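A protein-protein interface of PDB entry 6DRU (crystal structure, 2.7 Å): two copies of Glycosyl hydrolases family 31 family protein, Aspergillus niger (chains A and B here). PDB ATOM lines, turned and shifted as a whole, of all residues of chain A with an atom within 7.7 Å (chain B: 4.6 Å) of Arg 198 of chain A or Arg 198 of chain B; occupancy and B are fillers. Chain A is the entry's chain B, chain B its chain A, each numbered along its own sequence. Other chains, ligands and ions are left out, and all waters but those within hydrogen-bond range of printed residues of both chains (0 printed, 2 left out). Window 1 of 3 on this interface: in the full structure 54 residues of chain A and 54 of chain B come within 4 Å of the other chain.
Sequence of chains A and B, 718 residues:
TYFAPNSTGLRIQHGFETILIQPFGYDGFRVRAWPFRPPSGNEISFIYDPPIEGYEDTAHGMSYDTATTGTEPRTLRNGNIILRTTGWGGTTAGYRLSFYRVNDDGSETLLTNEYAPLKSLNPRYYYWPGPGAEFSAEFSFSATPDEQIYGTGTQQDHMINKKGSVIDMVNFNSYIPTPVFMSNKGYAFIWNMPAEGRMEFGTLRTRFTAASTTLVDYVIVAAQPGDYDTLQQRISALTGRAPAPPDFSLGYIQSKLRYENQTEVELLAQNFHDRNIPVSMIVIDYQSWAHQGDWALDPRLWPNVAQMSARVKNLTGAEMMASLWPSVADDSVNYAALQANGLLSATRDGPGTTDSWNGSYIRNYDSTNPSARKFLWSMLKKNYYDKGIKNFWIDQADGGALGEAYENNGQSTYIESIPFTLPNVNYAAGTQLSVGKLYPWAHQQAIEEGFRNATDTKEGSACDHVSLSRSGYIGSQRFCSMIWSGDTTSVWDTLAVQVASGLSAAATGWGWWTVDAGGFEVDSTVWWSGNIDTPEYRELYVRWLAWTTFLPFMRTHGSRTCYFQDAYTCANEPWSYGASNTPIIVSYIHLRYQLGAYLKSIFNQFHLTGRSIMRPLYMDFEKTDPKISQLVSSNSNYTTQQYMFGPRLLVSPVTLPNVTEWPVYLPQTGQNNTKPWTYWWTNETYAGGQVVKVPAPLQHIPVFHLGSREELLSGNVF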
ATOM      1  N   ALA A 137      25.566 -10.540  17.345  1.00  0.00           N
ATOM      2  CA  ALA A 137      25.225 -10.654  18.756  1.00  0.00           C
ATOM      3  C   ALA A 137      25.331 -12.101  19.212  1.00  0.00           C
ATOM      4  O   ALA A 137      24.966 -13.021  18.474  1.00  0.00           O
ATOM      5  CB  ALA A 137      23.810 -10.126  19.029  1.00  0.00           C
ATOM      6  N   GLU A 138      25.839 -12.295  20.429  1.00  0.00           N
ATOM      7  CA  GLU A 138      25.915 -13.608  21.065  1.00  0.00           C
ATOM      8  C   GLU A 138      25.416 -13.471  22.497  1.00  0.00           C
ATOM      9  O   GLU A 138      26.082 -12.852  23.335  1.00  0.00           O
ATOM     10  CB  GLU A 138      27.339 -14.166  21.038  1.00  0.00           C
ATOM     11  CG  GLU A 138      27.854 -14.514  19.652  1.00  0.00           C
ATOM     12  CD  GLU A 138      29.329 -14.872  19.651  1.00  0.00           C
ATOM     13  OE1 GLU A 138      29.695 -15.888  19.020  1.00  0.00           O
ATOM     14  OE2 GLU A 138      30.121 -14.149  20.291  1.00  0.00           O
ATOM     15  N   PHE A 139      24.251 -14.045  22.780  1.00  0.00           N
ATOM     16  CA  PHE A 139      23.628 -13.965  24.095  1.00  0.00           C
ATOM     17  C   PHE A 139      23.691 -15.326  24.776  1.00  0.00           C
ATOM     18  O   PHE A 139      23.289 -16.338  24.193  1.00  0.00           O
ATOM     19  CB  PHE A 139      22.179 -13.487  23.981  1.00  0.00           C
ATOM     20  CG  PHE A 139      22.035 -11.990  23.951  1.00  0.00           C
ATOM     21  CD1 PHE A 139      22.848 -11.215  23.139  1.00  0.00           C
ATOM     22  CD2 PHE A 139      21.085 -11.356  24.737  1.00  0.00           C
ATOM     23  CE1 PHE A 139      22.718  -9.838  23.112  1.00  0.00           C
ATOM     24  CE2 PHE A 139      20.950  -9.978  24.713  1.00  0.00           C
ATOM     25  CZ  PHE A 139      21.769  -9.219  23.900  1.00  0.00           C
ATOM     26  N   VAL A 166      23.855 -28.622  18.998  1.00  0.00           N
ATOM     27  CA  VAL A 166      23.945 -27.304  18.383  1.00  0.00           C
ATOM     28  C   VAL A 166      23.084 -27.319  17.129  1.00  0.00           C
ATOM     29  O   VAL A 166      23.233 -28.203  16.278  1.00  0.00           O
ATOM     30  CB  VAL A 166      25.397 -26.922  18.051  1.00  0.00           C
ATOM     31  CG1 VAL A 166      25.430 -25.606  17.291  1.00  0.00           C
ATOM     32  CG2 VAL A 166      26.212 -26.820  19.323  1.00  0.00           C
ATOM     33  N   ILE A 167      22.179 -26.351  17.021  1.00  0.00           N
ATOM     34  CA  ILE A 167      21.233 -26.276  15.916  1.00  0.00           C
ATOM     35  C   ILE A 167      21.542 -25.007  15.132  1.00  0.00           C
ATOM     36  O   ILE A 167      21.311 -23.893  15.622  1.00  0.00           O
ATOM     37  CB  ILE A 167      19.780 -26.290  16.404  1.00  0.00           C
ATOM     38  CG1 ILE A 167      19.449 -27.641  17.037  1.00  0.00           C
ATOM     39  CG2 ILE A 167      18.829 -26.025  15.248  1.00  0.00           C
ATOM     40  CD1 ILE A 167      18.473 -27.553  18.183  1.00  0.00           C
ATOM     41  N   ASP A 168      22.074 -25.171  13.924  1.00  0.00           N
ATOM     42  CA  ASP A 168      22.328 -24.032  13.056  1.00  0.00           C
ATOM     43  C   ASP A 168      21.019 -23.484  12.505  1.00  0.00           C
ATOM     44  O   ASP A 168      20.125 -24.242  12.119  1.00  0.00           O
ATOM     45  CB  ASP A 168      23.254 -24.433  11.909  1.00  0.00           C
ATOM     46  CG  ASP A 168      24.496 -25.159  12.387  1.00  0.00           C
ATOM     47  OD1 ASP A 168      25.180 -24.636  13.290  1.00  0.00           O
ATOM     48  OD2 ASP A 168      24.784 -26.256  11.862  1.00  0.00           O
ATOM     49  N   MET A 169      20.906 -22.157  12.467  1.00  0.00           N
ATOM     50  CA  MET A 169      19.698 -21.502  11.962  1.00  0.00           C
ATOM     51  C   MET A 169      19.888 -21.162  10.482  1.00  0.00           C
ATOM     52  O   MET A 169      19.967 -20.005  10.069  1.00  0.00           O
ATOM     53  CB  MET A 169      19.374 -20.272  12.800  1.00  0.00           C
ATOM     54  CG  MET A 169      18.834 -20.620  14.175  1.00  0.00           C
ATOM     55  SD  MET A 169      18.068 -19.236  15.030  1.00  0.00           S
ATOM     56  CE  MET A 169      19.462 -18.599  15.956  1.00  0.00           C
ATOM     57  N   VAL A 170      19.959 -22.224   9.681  1.00  0.00           N
ATOM     58  CA  VAL A 170      20.069 -22.134   8.227  1.00  0.00           C
ATOM     59  C   VAL A 170      19.103 -23.148   7.634  1.00  0.00           C
ATOM     60  O   VAL A 170      19.188 -24.341   7.948  1.00  0.00           O
ATOM     61  CB  VAL A 170      21.500 -22.415   7.731  1.00  0.00           C
ATOM     62  CG1 VAL A 170      21.574 -22.274   6.221  1.00  0.00           C
ATOM     63  CG2 VAL A 170      22.501 -21.500   8.413  1.00  0.00           C
ATOM     64  N   PRO A 179      13.937 -20.988  16.748  1.00  0.00           N
ATOM     65  CA  PRO A 179      14.342 -20.799  18.153  1.00  0.00           C
ATOM     66  C   PRO A 179      13.160 -20.562  19.091  1.00  0.00           C
ATOM     67  O   PRO A 179      13.001 -19.493  19.688  1.00  0.00           O
ATOM     68  CB  PRO A 179      15.275 -19.586  18.057  1.00  0.00           C
ATOM     69  CG  PRO A 179      14.719 -18.789  16.930  1.00  0.00           C
ATOM     70  CD  PRO A 179      14.185 -19.787  15.932  1.00  0.00           C
ATOM     71  N   TRP A 191      13.387 -16.761  20.758  1.00  0.00           N
ATOM     72  CA  TRP A 191      14.427 -15.878  20.230  1.00  0.00           C
ATOM     73  C   TRP A 191      13.822 -15.176  19.020  1.00  0.00           C
ATOM     74  O   TRP A 191      13.904 -15.653  17.887  1.00  0.00           O
ATOM     75  CB  TRP A 191      15.676 -16.684  19.888  1.00  0.00           C
ATOM     76  CG  TRP A 191      16.850 -15.911  19.352  1.00  0.00           C
ATOM     77  CD1 TRP A 191      17.273 -15.863  18.055  1.00  0.00           C
ATOM     78  CD2 TRP A 191      17.779 -15.118  20.105  1.00  0.00           C
ATOM     79  NE1 TRP A 191      18.395 -15.077  17.951  1.00  0.00           N
ATOM     80  CE2 TRP A 191      18.724 -14.607  19.194  1.00  0.00           C
ATOM     81  CE3 TRP A 191      17.895 -14.783  21.458  1.00  0.00           C
ATOM     82  CZ2 TRP A 191      19.770 -13.777  19.591  1.00  0.00           C
ATOM     83  CZ3 TRP A 191      18.936 -13.959  21.850  1.00  0.00           C
ATOM     84  CH2 TRP A 191      19.860 -13.468  20.920  1.00  0.00           C
ATOM     85  N   ALA A 195      17.337 -13.184  11.985  1.00  0.00           N
ATOM     86  CA  ALA A 195      18.693 -13.357  11.492  1.00  0.00           C
ATOM     87  C   ALA A 195      19.122 -14.816  11.574  1.00  0.00           C
ATOM     88  O   ALA A 195      18.710 -15.558  12.470  1.00  0.00           O
ATOM     89  CB  ALA A 195      19.668 -12.491  12.291  1.00  0.00           C
ATOM     90  N   GLU A 196      19.950 -15.225  10.617  1.00  0.00           N
ATOM     91  CA  GLU A 196      20.587 -16.530  10.698  1.00  0.00           C
ATOM     92  C   GLU A 196      21.577 -16.555  11.854  1.00  0.00           C
ATOM     93  O   GLU A 196      22.105 -15.520  12.274  1.00  0.00           O
ATOM     94  CB  GLU A 196      21.302 -16.867   9.389  1.00  0.00           C
ATOM     95  CG  GLU A 196      20.368 -17.100   8.215  1.00  0.00           C
ATOM     96  CD  GLU A 196      21.073 -17.717   7.021  1.00  0.00           C
ATOM     97  OE1 GLU A 196      22.321 -17.696   6.989  1.00  0.00           O
ATOM     98  OE2 GLU A 196      20.377 -18.221   6.114  1.00  0.00           O
ATOM     99  N   GLY A 197      21.830 -17.750  12.373  1.00  0.00           N
ATOM    100  CA  GLY A 197      22.724 -17.866  13.505  1.00  0.00           C
ATOM    101  C   GLY A 197      22.946 -19.275  14.008  1.00  0.00           C
ATOM    102  O   GLY A 197      23.263 -20.183  13.234  1.00  0.00           O
ATOM    103  N   ARG A 198      22.762 -19.466  15.312  1.00  0.00           N
ATOM    104  CA  ARG A 198      23.210 -20.678  15.979  1.00  0.00           C
ATOM    105  C   ARG A 198      22.423 -20.855  17.269  1.00  0.00           C
ATOM    106  O   ARG A 198      22.143 -19.880  17.972  1.00  0.00           O
ATOM    107  CB  ARG A 198      24.712 -20.596  16.275  1.00  0.00           C
ATOM    108  CG  ARG A 198      25.378 -21.892  16.674  1.00  0.00           C
ATOM    109  CD  ARG A 198      26.703 -21.596  17.362  1.00  0.00           C
ATOM    110  NE  ARG A 198      27.436 -20.522  16.695  1.00  0.00           N
ATOM    111  CZ  ARG A 198      28.293 -19.709  17.305  1.00  0.00           C
ATOM    112  NH1 ARG A 198      28.525 -19.836  18.604  1.00  0.00           N
ATOM    113  NH2 ARG A 198      28.913 -18.760  16.617  1.00  0.00           N
ATOM    114  N   MET A 199      22.065 -22.101  17.565  1.00  0.00           N
ATOM    115  CA  MET A 199      21.446 -22.474  18.831  1.00  0.00           C
ATOM    116  C   MET A 199      22.379 -23.445  19.539  1.00  0.00           C
ATOM    117  O   MET A 199      22.641 -24.537  19.027  1.00  0.00           O
ATOM    118  CB  MET A 199      20.073 -23.117  18.615  1.00  0.00           C
ATOM    119  CG  MET A 199      18.912 -22.139  18.529  1.00  0.00           C
ATOM    120  SD  MET A 199      17.322 -22.969  18.310  1.00  0.00           S
ATOM    121  CE  MET A 199      17.210 -23.080  16.526  1.00  0.00           C
ATOM    122  N   GLU A 200      22.883 -23.049  20.703  1.00  0.00           N
ATOM    123  CA  GLU A 200      23.763 -23.892  21.508  1.00  0.00           C
ATOM    124  C   GLU A 200      23.029 -24.298  22.779  1.00  0.00           C
ATOM    125  O   GLU A 200      22.818 -23.470  23.671  1.00  0.00           O
ATOM    126  CB  GLU A 200      25.064 -23.173  21.855  1.00  0.00           C
ATOM    127  CG  GLU A 200      25.934 -22.816  20.674  1.00  0.00           C
ATOM    128  CD  GLU A 200      27.235 -22.172  21.107  1.00  0.00           C
ATOM    129  OE1 GLU A 200      27.471 -22.072  22.329  1.00  0.00           O
ATOM    130  OE2 GLU A 200      28.019 -21.760  20.228  1.00  0.00           O
ATOM    131  N   PHE A 201      22.646 -25.569  22.866  1.00  0.00           N
ATOM    132  CA  PHE A 201      22.040 -26.101  24.084  1.00  0.00           C
ATOM    133  C   PHE A 201      23.069 -26.946  24.833  1.00  0.00           C
ATOM    134  O   PHE A 201      22.976 -28.169  24.936  1.00  0.00           O
ATOM    135  CB  PHE A 201      20.779 -26.889  23.749  1.00  0.00           C
ATOM    136  CG  PHE A 201      19.666 -26.038  23.209  1.00  0.00           C
ATOM    137  CD1 PHE A 201      18.956 -25.194  24.048  1.00  0.00           C
ATOM    138  CD2 PHE A 201      19.330 -26.079  21.867  1.00  0.00           C
ATOM    139  CE1 PHE A 201      17.932 -24.402  23.556  1.00  0.00           C
ATOM    140  CE2 PHE A 201      18.306 -25.292  21.369  1.00  0.00           C
ATOM    141  CZ  PHE A 201      17.605 -24.453  22.215  1.00  0.00           C
ATOM    142  N   ARG A 205      25.527 -23.926  29.485  1.00  0.00           N
ATOM    143  CA  ARG A 205      25.282 -22.629  28.869  1.00  0.00           C
ATOM    144  C   ARG A 205      24.411 -22.796  27.633  1.00  0.00           C
ATOM    145  O   ARG A 205      24.681 -23.654  26.788  1.00  0.00           O
ATOM    146  CB  ARG A 205      26.608 -21.945  28.515  1.00  0.00           C
ATOM    147  CG  ARG A 205      26.480 -20.633  27.762  1.00  0.00           C
ATOM    148  CD  ARG A 205      27.859 -20.041  27.512  1.00  0.00           C
ATOM    149  NE  ARG A 205      28.672 -20.869  26.626  1.00  0.00           N
ATOM    150  CZ  ARG A 205      29.026 -20.522  25.394  1.00  0.00           C
ATOM    151  NH1 ARG A 205      28.645 -19.354  24.901  1.00  0.00           N
ATOM    152  NH2 ARG A 205      29.765 -21.339  24.657  1.00  0.00           N
ATOM    153  N   ARG A 207      23.174 -20.661  24.351  1.00  0.00           N
ATOM    154  CA  ARG A 207      23.631 -19.505  23.594  1.00  0.00           C
ATOM    155  C   ARG A 207      22.872 -19.383  22.281  1.00  0.00           C
ATOM    156  O   ARG A 207      22.740 -20.362  21.540  1.00  0.00           O
ATOM    157  CB  ARG A 207      25.134 -19.585  23.317  1.00  0.00           C
ATOM    158  CG  ARG A 207      25.672 -18.372  22.577  1.00  0.00           C
ATOM    159  CD  ARG A 207      27.169 -18.454  22.376  1.00  0.00           C
ATOM    160  NE  ARG A 207      27.879 -17.471  23.188  1.00  0.00           N
ATOM    161  CZ  ARG A 207      29.176 -17.208  23.078  1.00  0.00           C
ATOM    162  NH1 ARG A 207      29.911 -17.856  22.184  1.00  0.00           N
ATOM    163  NH2 ARG A 207      29.738 -16.297  23.862  1.00  0.00           N
ATOM    164  N   PHE A 208      22.380 -18.178  22.004  1.00  0.00           N
ATOM    165  CA  PHE A 208      21.795 -17.821  20.720  1.00  0.00           C
ATOM    166  C   PHE A 208      22.653 -16.743  20.073  1.00  0.00           C
ATOM    167  O   PHE A 208      23.160 -15.849  20.757  1.00  0.00           O
ATOM    168  CB  PHE A 208      20.361 -17.311  20.879  1.00  0.00           C
ATOM    169  CG  PHE A 208      19.417 -18.325  21.446  1.00  0.00           C
ATOM    170  CD1 PHE A 208      19.270 -18.467  22.816  1.00  0.00           C
ATOM    171  CD2 PHE A 208      18.670 -19.133  20.608  1.00  0.00           C
ATOM    172  CE1 PHE A 208      18.398 -19.402  23.338  1.00  0.00           C
ATOM    173  CE2 PHE A 208      17.795 -20.067  21.123  1.00  0.00           C
ATOM    174  CZ  PHE A 208      17.660 -20.203  22.491  1.00  0.00           C
ATOM    175  N   THR A 209      22.814 -16.826  18.754  1.00  0.00           N
ATOM    176  CA  THR A 209      23.620 -15.864  18.017  1.00  0.00           C
ATOM    177  C   THR A 209      22.832 -15.310  16.839  1.00  0.00           C
ATOM    178  O   THR A 209      21.913 -15.952  16.323  1.00  0.00           O
ATOM    179  CB  THR A 209      24.929 -16.487  17.498  1.00  0.00           C
ATOM    180  OG1 THR A 209      24.634 -17.433  16.464  1.00  0.00           O
ATOM    181  CG2 THR A 209      25.677 -17.192  18.619  1.00  0.00           C
ATOM    182  N   ALA A 210      23.206 -14.103  16.422  1.00  0.00           N
ATOM    183  CA  ALA A 210      22.636 -13.452  15.249  1.00  0.00           C
ATOM    184  C   ALA A 210      23.787 -12.931  14.403  1.00  0.00           C
ATOM    185  O   ALA A 210      24.629 -12.177  14.900  1.00  0.00           O
ATOM    186  CB  ALA A 210      21.690 -12.316  15.645  1.00  0.00           C
ATOM    187  N   ALA A 211      23.827 -13.338  13.130  1.00  0.00           N
ATOM    188  CA  ALA A 211      24.943 -12.966  12.266  1.00  0.00           C
ATOM    189  C   ALA A 211      25.003 -11.458  12.054  1.00  0.00           C
ATOM    190  O   ALA A 211      26.085 -10.859  12.085  1.00  0.00           O
ATOM    191  CB  ALA A 211      24.834 -13.690  10.925  1.00  0.00           C
ATOM    192  N   GLU B 138      34.458 -24.133   8.583  1.00  0.00           N
ATOM    193  CA  GLU B 138      33.629 -24.920   9.490  1.00  0.00           C
ATOM    194  C   GLU B 138      33.689 -26.371   9.034  1.00  0.00           C
ATOM    195  O   GLU B 138      33.120 -26.719   7.994  1.00  0.00           O
ATOM    196  CB  GLU B 138      32.188 -24.405   9.502  1.00  0.00           C
ATOM    197  CG  GLU B 138      32.036 -23.024  10.122  1.00  0.00           C
ATOM    198  CD  GLU B 138      30.659 -22.427   9.898  1.00  0.00           C
ATOM    199  OE1 GLU B 138      30.543 -21.457   9.115  1.00  0.00           O
ATOM    200  OE2 GLU B 138      29.692 -22.930  10.501  1.00  0.00           O
ATOM    201  N   VAL B 166      29.925 -26.745  24.226  1.00  0.00           N
ATOM    202  CA  VAL B 166      30.551 -25.893  23.223  1.00  0.00           C
ATOM    203  C   VAL B 166      31.670 -25.122  23.901  1.00  0.00           C
ATOM    204  O   VAL B 166      31.450 -24.476  24.934  1.00  0.00           O
ATOM    205  CB  VAL B 166      29.540 -24.937  22.571  1.00  0.00           C
ATOM    206  CG1 VAL B 166      30.254 -23.981  21.630  1.00  0.00           C
ATOM    207  CG2 VAL B 166      28.484 -25.726  21.827  1.00  0.00           C
ATOM    208  N   ILE B 167      32.869 -25.198  23.335  1.00  0.00           N
ATOM    209  CA  ILE B 167      34.052 -24.564  23.906  1.00  0.00           C
ATOM    210  C   ILE B 167      34.537 -23.506  22.925  1.00  0.00           C
ATOM    211  O   ILE B 167      35.046 -23.836  21.846  1.00  0.00           O
ATOM    212  CB  ILE B 167      35.156 -25.580  24.216  1.00  0.00           C
ATOM    213  CG1 ILE B 167      34.713 -26.510  25.344  1.00  0.00           C
ATOM    214  CG2 ILE B 167      36.437 -24.868  24.607  1.00  0.00           C
ATOM    215  CD1 ILE B 167      35.248 -27.911  25.220  1.00  0.00           C
ATOM    216  N   ASP B 168      34.375 -22.237  23.292  1.00  0.00           N
ATOM    217  CA  ASP B 168      34.895 -21.150  22.479  1.00  0.00           C
ATOM    218  C   ASP B 168      36.413 -21.092  22.596  1.00  0.00           C
ATOM    219  O   ASP B 168      36.973 -21.241  23.685  1.00  0.00           O
ATOM    220  CB  ASP B 168      34.283 -19.820  22.912  1.00  0.00           C
ATOM    221  CG  ASP B 168      32.773 -19.876  23.005  1.00  0.00           C
ATOM    222  OD1 ASP B 168      32.135 -20.308  22.022  1.00  0.00           O
ATOM    223  OD2 ASP B 168      32.225 -19.496  24.063  1.00  0.00           O
ATOM    224  N   MET B 169      37.082 -20.872  21.467  1.00  0.00           N
ATOM    225  CA  MET B 169      38.543 -20.808  21.444  1.00  0.00           C
ATOM    226  C   MET B 169      39.009 -19.356  21.546  1.00  0.00           C
ATOM    227  O   MET B 169      39.576 -18.776  20.620  1.00  0.00           O
ATOM    228  CB  MET B 169      39.083 -21.490  20.194  1.00  0.00           C
ATOM    229  CG  MET B 169      38.979 -23.002  20.241  1.00  0.00           C
ATOM    230  SD  MET B 169      40.002 -23.789  18.988  1.00  0.00           S
ATOM    231  CE  MET B 169      38.833 -23.923  17.642  1.00  0.00           C
ATOM    232  N   GLY B 197      38.110 -19.609  17.363  1.00  0.00           N
ATOM    233  CA  GLY B 197      36.957 -20.276  16.798  1.00  0.00           C
ATOM    234  C   GLY B 197      36.032 -20.915  17.809  1.00  0.00           C
ATOM    235  O   GLY B 197      35.608 -20.275  18.776  1.00  0.00           O
ATOM    236  N   ARG B 198      35.719 -22.190  17.598  1.00  0.00           N
ATOM    237  CA  ARG B 198      34.629 -22.826  18.316  1.00  0.00           C
ATOM    238  C   ARG B 198      34.824 -24.332  18.294  1.00  0.00           C
ATOM    239  O   ARG B 198      35.240 -24.897  17.278  1.00  0.00           O
ATOM    240  CB  ARG B 198      33.288 -22.449  17.680  1.00  0.00           C
ATOM    241  CG  ARG B 198      32.057 -22.768  18.494  1.00  0.00           C
ATOM    242  CD  ARG B 198      30.841 -22.772  17.581  1.00  0.00           C
ATOM    243  NE  ARG B 198      30.885 -21.673  16.620  1.00  0.00           N
ATOM    244  CZ  ARG B 198      30.315 -21.704  15.420  1.00  0.00           C
ATOM    245  NH1 ARG B 198      29.657 -22.784  15.024  1.00  0.00           N
ATOM    246  NH2 ARG B 198      30.409 -20.658  14.611  1.00  0.00           N
ATOM    247  N   MET B 199      34.520 -24.973  19.418  1.00  0.00           N
ATOM    248  CA  MET B 199      34.497 -26.425  19.530  1.00  0.00           C
ATOM    249  C   MET B 199      33.076 -26.849  19.867  1.00  0.00           C
ATOM    250  O   MET B 199      32.557 -26.488  20.928  1.00  0.00           O
ATOM    251  CB  MET B 199      35.473 -26.915  20.603  1.00  0.00           C
ATOM    252  CG  MET B 199      36.891 -27.146  20.115  1.00  0.00           C
ATOM    253  SD  MET B 199      37.981 -27.752  21.425  1.00  0.00           S
ATOM    254  CE  MET B 199      38.602 -26.222  22.116  1.00  0.00           C
ATOM    255  N   GLU B 200      32.446 -27.604  18.970  1.00  0.00           N
ATOM    256  CA  GLU B 200      31.091 -28.110  19.176  1.00  0.00           C
ATOM    257  C   GLU B 200      31.152 -29.622  19.347  1.00  0.00           C
ATOM    258  O   GLU B 200      31.382 -30.352  18.377  1.00  0.00           O
ATOM    259  CB  GLU B 200      30.177 -27.747  18.009  1.00  0.00           C
ATOM    260  CG  GLU B 200      29.952 -26.269  17.805  1.00  0.00           C
ATOM    261  CD  GLU B 200      28.986 -25.995  16.670  1.00  0.00           C
ATOM    262  OE1 GLU B 200      28.454 -26.970  16.095  1.00  0.00           O
ATOM    263  OE2 GLU B 200      28.763 -24.810  16.346  1.00  0.00           O
ATOM    264  N   ARG B 207      32.114 -30.360  15.522  1.00  0.00           N
ATOM    265  CA  ARG B 207      32.407 -29.279  14.590  1.00  0.00           C
ATOM    266  C   ARG B 207      33.494 -28.371  15.146  1.00  0.00           C
ATOM    267  O   ARG B 207      33.413 -27.927  16.295  1.00  0.00           O
ATOM    268  CB  ARG B 207      31.152 -28.457  14.283  1.00  0.00           C
ATOM    269  CG  ARG B 207      31.392 -27.351  13.277  1.00  0.00           C
ATOM    270  CD  ARG B 207      30.114 -26.606  12.952  1.00  0.00           C
ATOM    271  NE  ARG B 207      29.668 -26.869  11.588  1.00  0.00           N
ATOM    272  CZ  ARG B 207      28.683 -26.212  10.984  1.00  0.00           C
ATOM    273  NH1 ARG B 207      28.040 -25.246  11.627  1.00  0.00           N
ATOM    274  NH2 ARG B 207      28.343 -26.517   9.740  1.00  0.00           N
ATOM    275  N   PHE B 208      34.499 -28.093  14.320  1.00  0.00           N
ATOM    276  CA  PHE B 208      35.537 -27.116  14.615  1.00  0.00           C
ATOM    277  C   PHE B 208      35.452 -25.984  13.604  1.00  0.00           C
ATOM    278  O   PHE B 208      35.180 -26.219  12.421  1.00  0.00           O
ATOM    279  CB  PHE B 208      36.928 -27.751  14.574  1.00  0.00           C
ATOM    280  CG  PHE B 208      37.126 -28.840  15.584  1.00  0.00           C
ATOM    281  CD1 PHE B 208      36.777 -30.149  15.290  1.00  0.00           C
ATOM    282  CD2 PHE B 208      37.658 -28.558  16.831  1.00  0.00           C
ATOM    283  CE1 PHE B 208      36.957 -31.157  16.221  1.00  0.00           C
ATOM    284  CE2 PHE B 208      37.841 -29.559  17.767  1.00  0.00           C
ATOM    285  CZ  PHE B 208      37.488 -30.862  17.461  1.00  0.00           C
ATOM    286  N   THR B 209      35.685 -24.756  14.066  1.00  0.00           N
ATOM    287  CA  THR B 209      35.629 -23.585  13.202  1.00  0.00           C
ATOM    288  C   THR B 209      36.905 -22.766  13.346  1.00  0.00           C
ATOM    289  O   THR B 209      37.589 -22.821  14.372  1.00  0.00           O
ATOM    290  CB  THR B 209      34.417 -22.687  13.511  1.00  0.00           C
ATOM    291  OG1 THR B 209      34.593 -22.057  14.785  1.00  0.00           O
ATOM    292  CG2 THR B 209      33.129 -23.499  13.523  1.00  0.00           C
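Of the 12 printed residues of chain B, 5 touch a printed residue of chain A.
Printed residues of chain B that touch a printed residue of chain A: Val 166, Asp 168, Arg 198, Glu 200 and Arg 207.
Printed residues of chain A that touch a printed residue of chain B: Val 166, Asp 168, Arg 198, Glu 200, Arg 205 and Arg 207.
Hydrophobic or aromatic side chains of chain A within 4 Å of the printed part of chain B: Val 166.
Among the printed residues, 10 pairs touch across the chains.
Among the printed residues, Asp or Glu carboxylates within 4 Å of a Lys or Arg side-chain nitrogen of the other chain: Asp 168 of chain A with Arg 207 of chain B, Arg 205 of chain A with Asp 168 of chain B and Arg 207 of chain A with Asp 168 of chain B.
NH1 of Arg 207 of chain B lies within salt-bridge range of OD1 of Asp 168 of chain A (3.4 Å).
The guanidinium group (NH2) of Arg 198 of chain A sits close to the guanidinium group (NH2) of Arg 198 of chain B (3.1 Å).
The side-chain carboxylate (OD2) of Asp 168 of chain B lies within salt-bridge range of the guanidinium group (NH2) of Arg 205 of chain A (3.1 Å).
The guanidinium group (NH1) of Arg 207 of chain A lies within salt-bridge range of the side-chain carboxylate (OD1) of Asp 168 of chain B, 3.3 Å away.
Among the printed residues, merely in contact across the chains: Val 166 of chain A with Val 166 of chain B, Val 166 of chain A with Glu 200 of chain B, Arg 198 of chain A with Glu 200 of chain B, Glu 200 of chain A with Val 166 of chain B, Glu 200 of chain A with Arg 198 of chain B and Arg 205 of chain A with Val 166 of chain B.
The guanidinium group of Arg 198 of chain A is in salt-bridge range of the side-chain carboxylate of Glu 138 of chain A (3.8 Å).
The side-chain carboxylate (OE2) of Glu 138 of chain B lies within salt-bridge range of the guanidinium group (NH1) of Arg 207 of chain B, 3.1 Å away.
The side-chain carboxylate of Glu 138 of chain A is in salt-bridge range of the guanidinium group of Arg 207 of chain A, at 3.7 Å.
Arg 198 of chain A touches two residues of chain B.
Of the printed residues of chain A, Arg 198 of chain B touches Arg 198 (3.1 Å) and Glu 200 (3.999 Å).
Of the printed residues of chain B, Glu 200 of chain A touches Val 166 and Arg 198.
Printed residues of chain B within 4 Å of Arg 207 of chain A: Asp 168 (3.3 Å).
Printed residues of chain A within 4 Å of Arg 207 of chain B: Asp 168.
The nearest printed residue of chain A that does not touch Arg 207 of chain B is Val 166 of chain A (6.2 Å).
Val 166 of chain A touches its own counterpart, Val 166 of chain B.
Asp 168 of chain A touches Arg 207 of chain B, and with the chains exchanged Arg 207 of chain A touches Asp 168 of chain B.
Arg 198 of chain B touches its own counterpart, Arg 198 of chain A.
Arg 198 of chain A touches Glu 200 of chain B, and with the chains exchanged Glu 200 of chain A touches Arg 198 of chain B.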
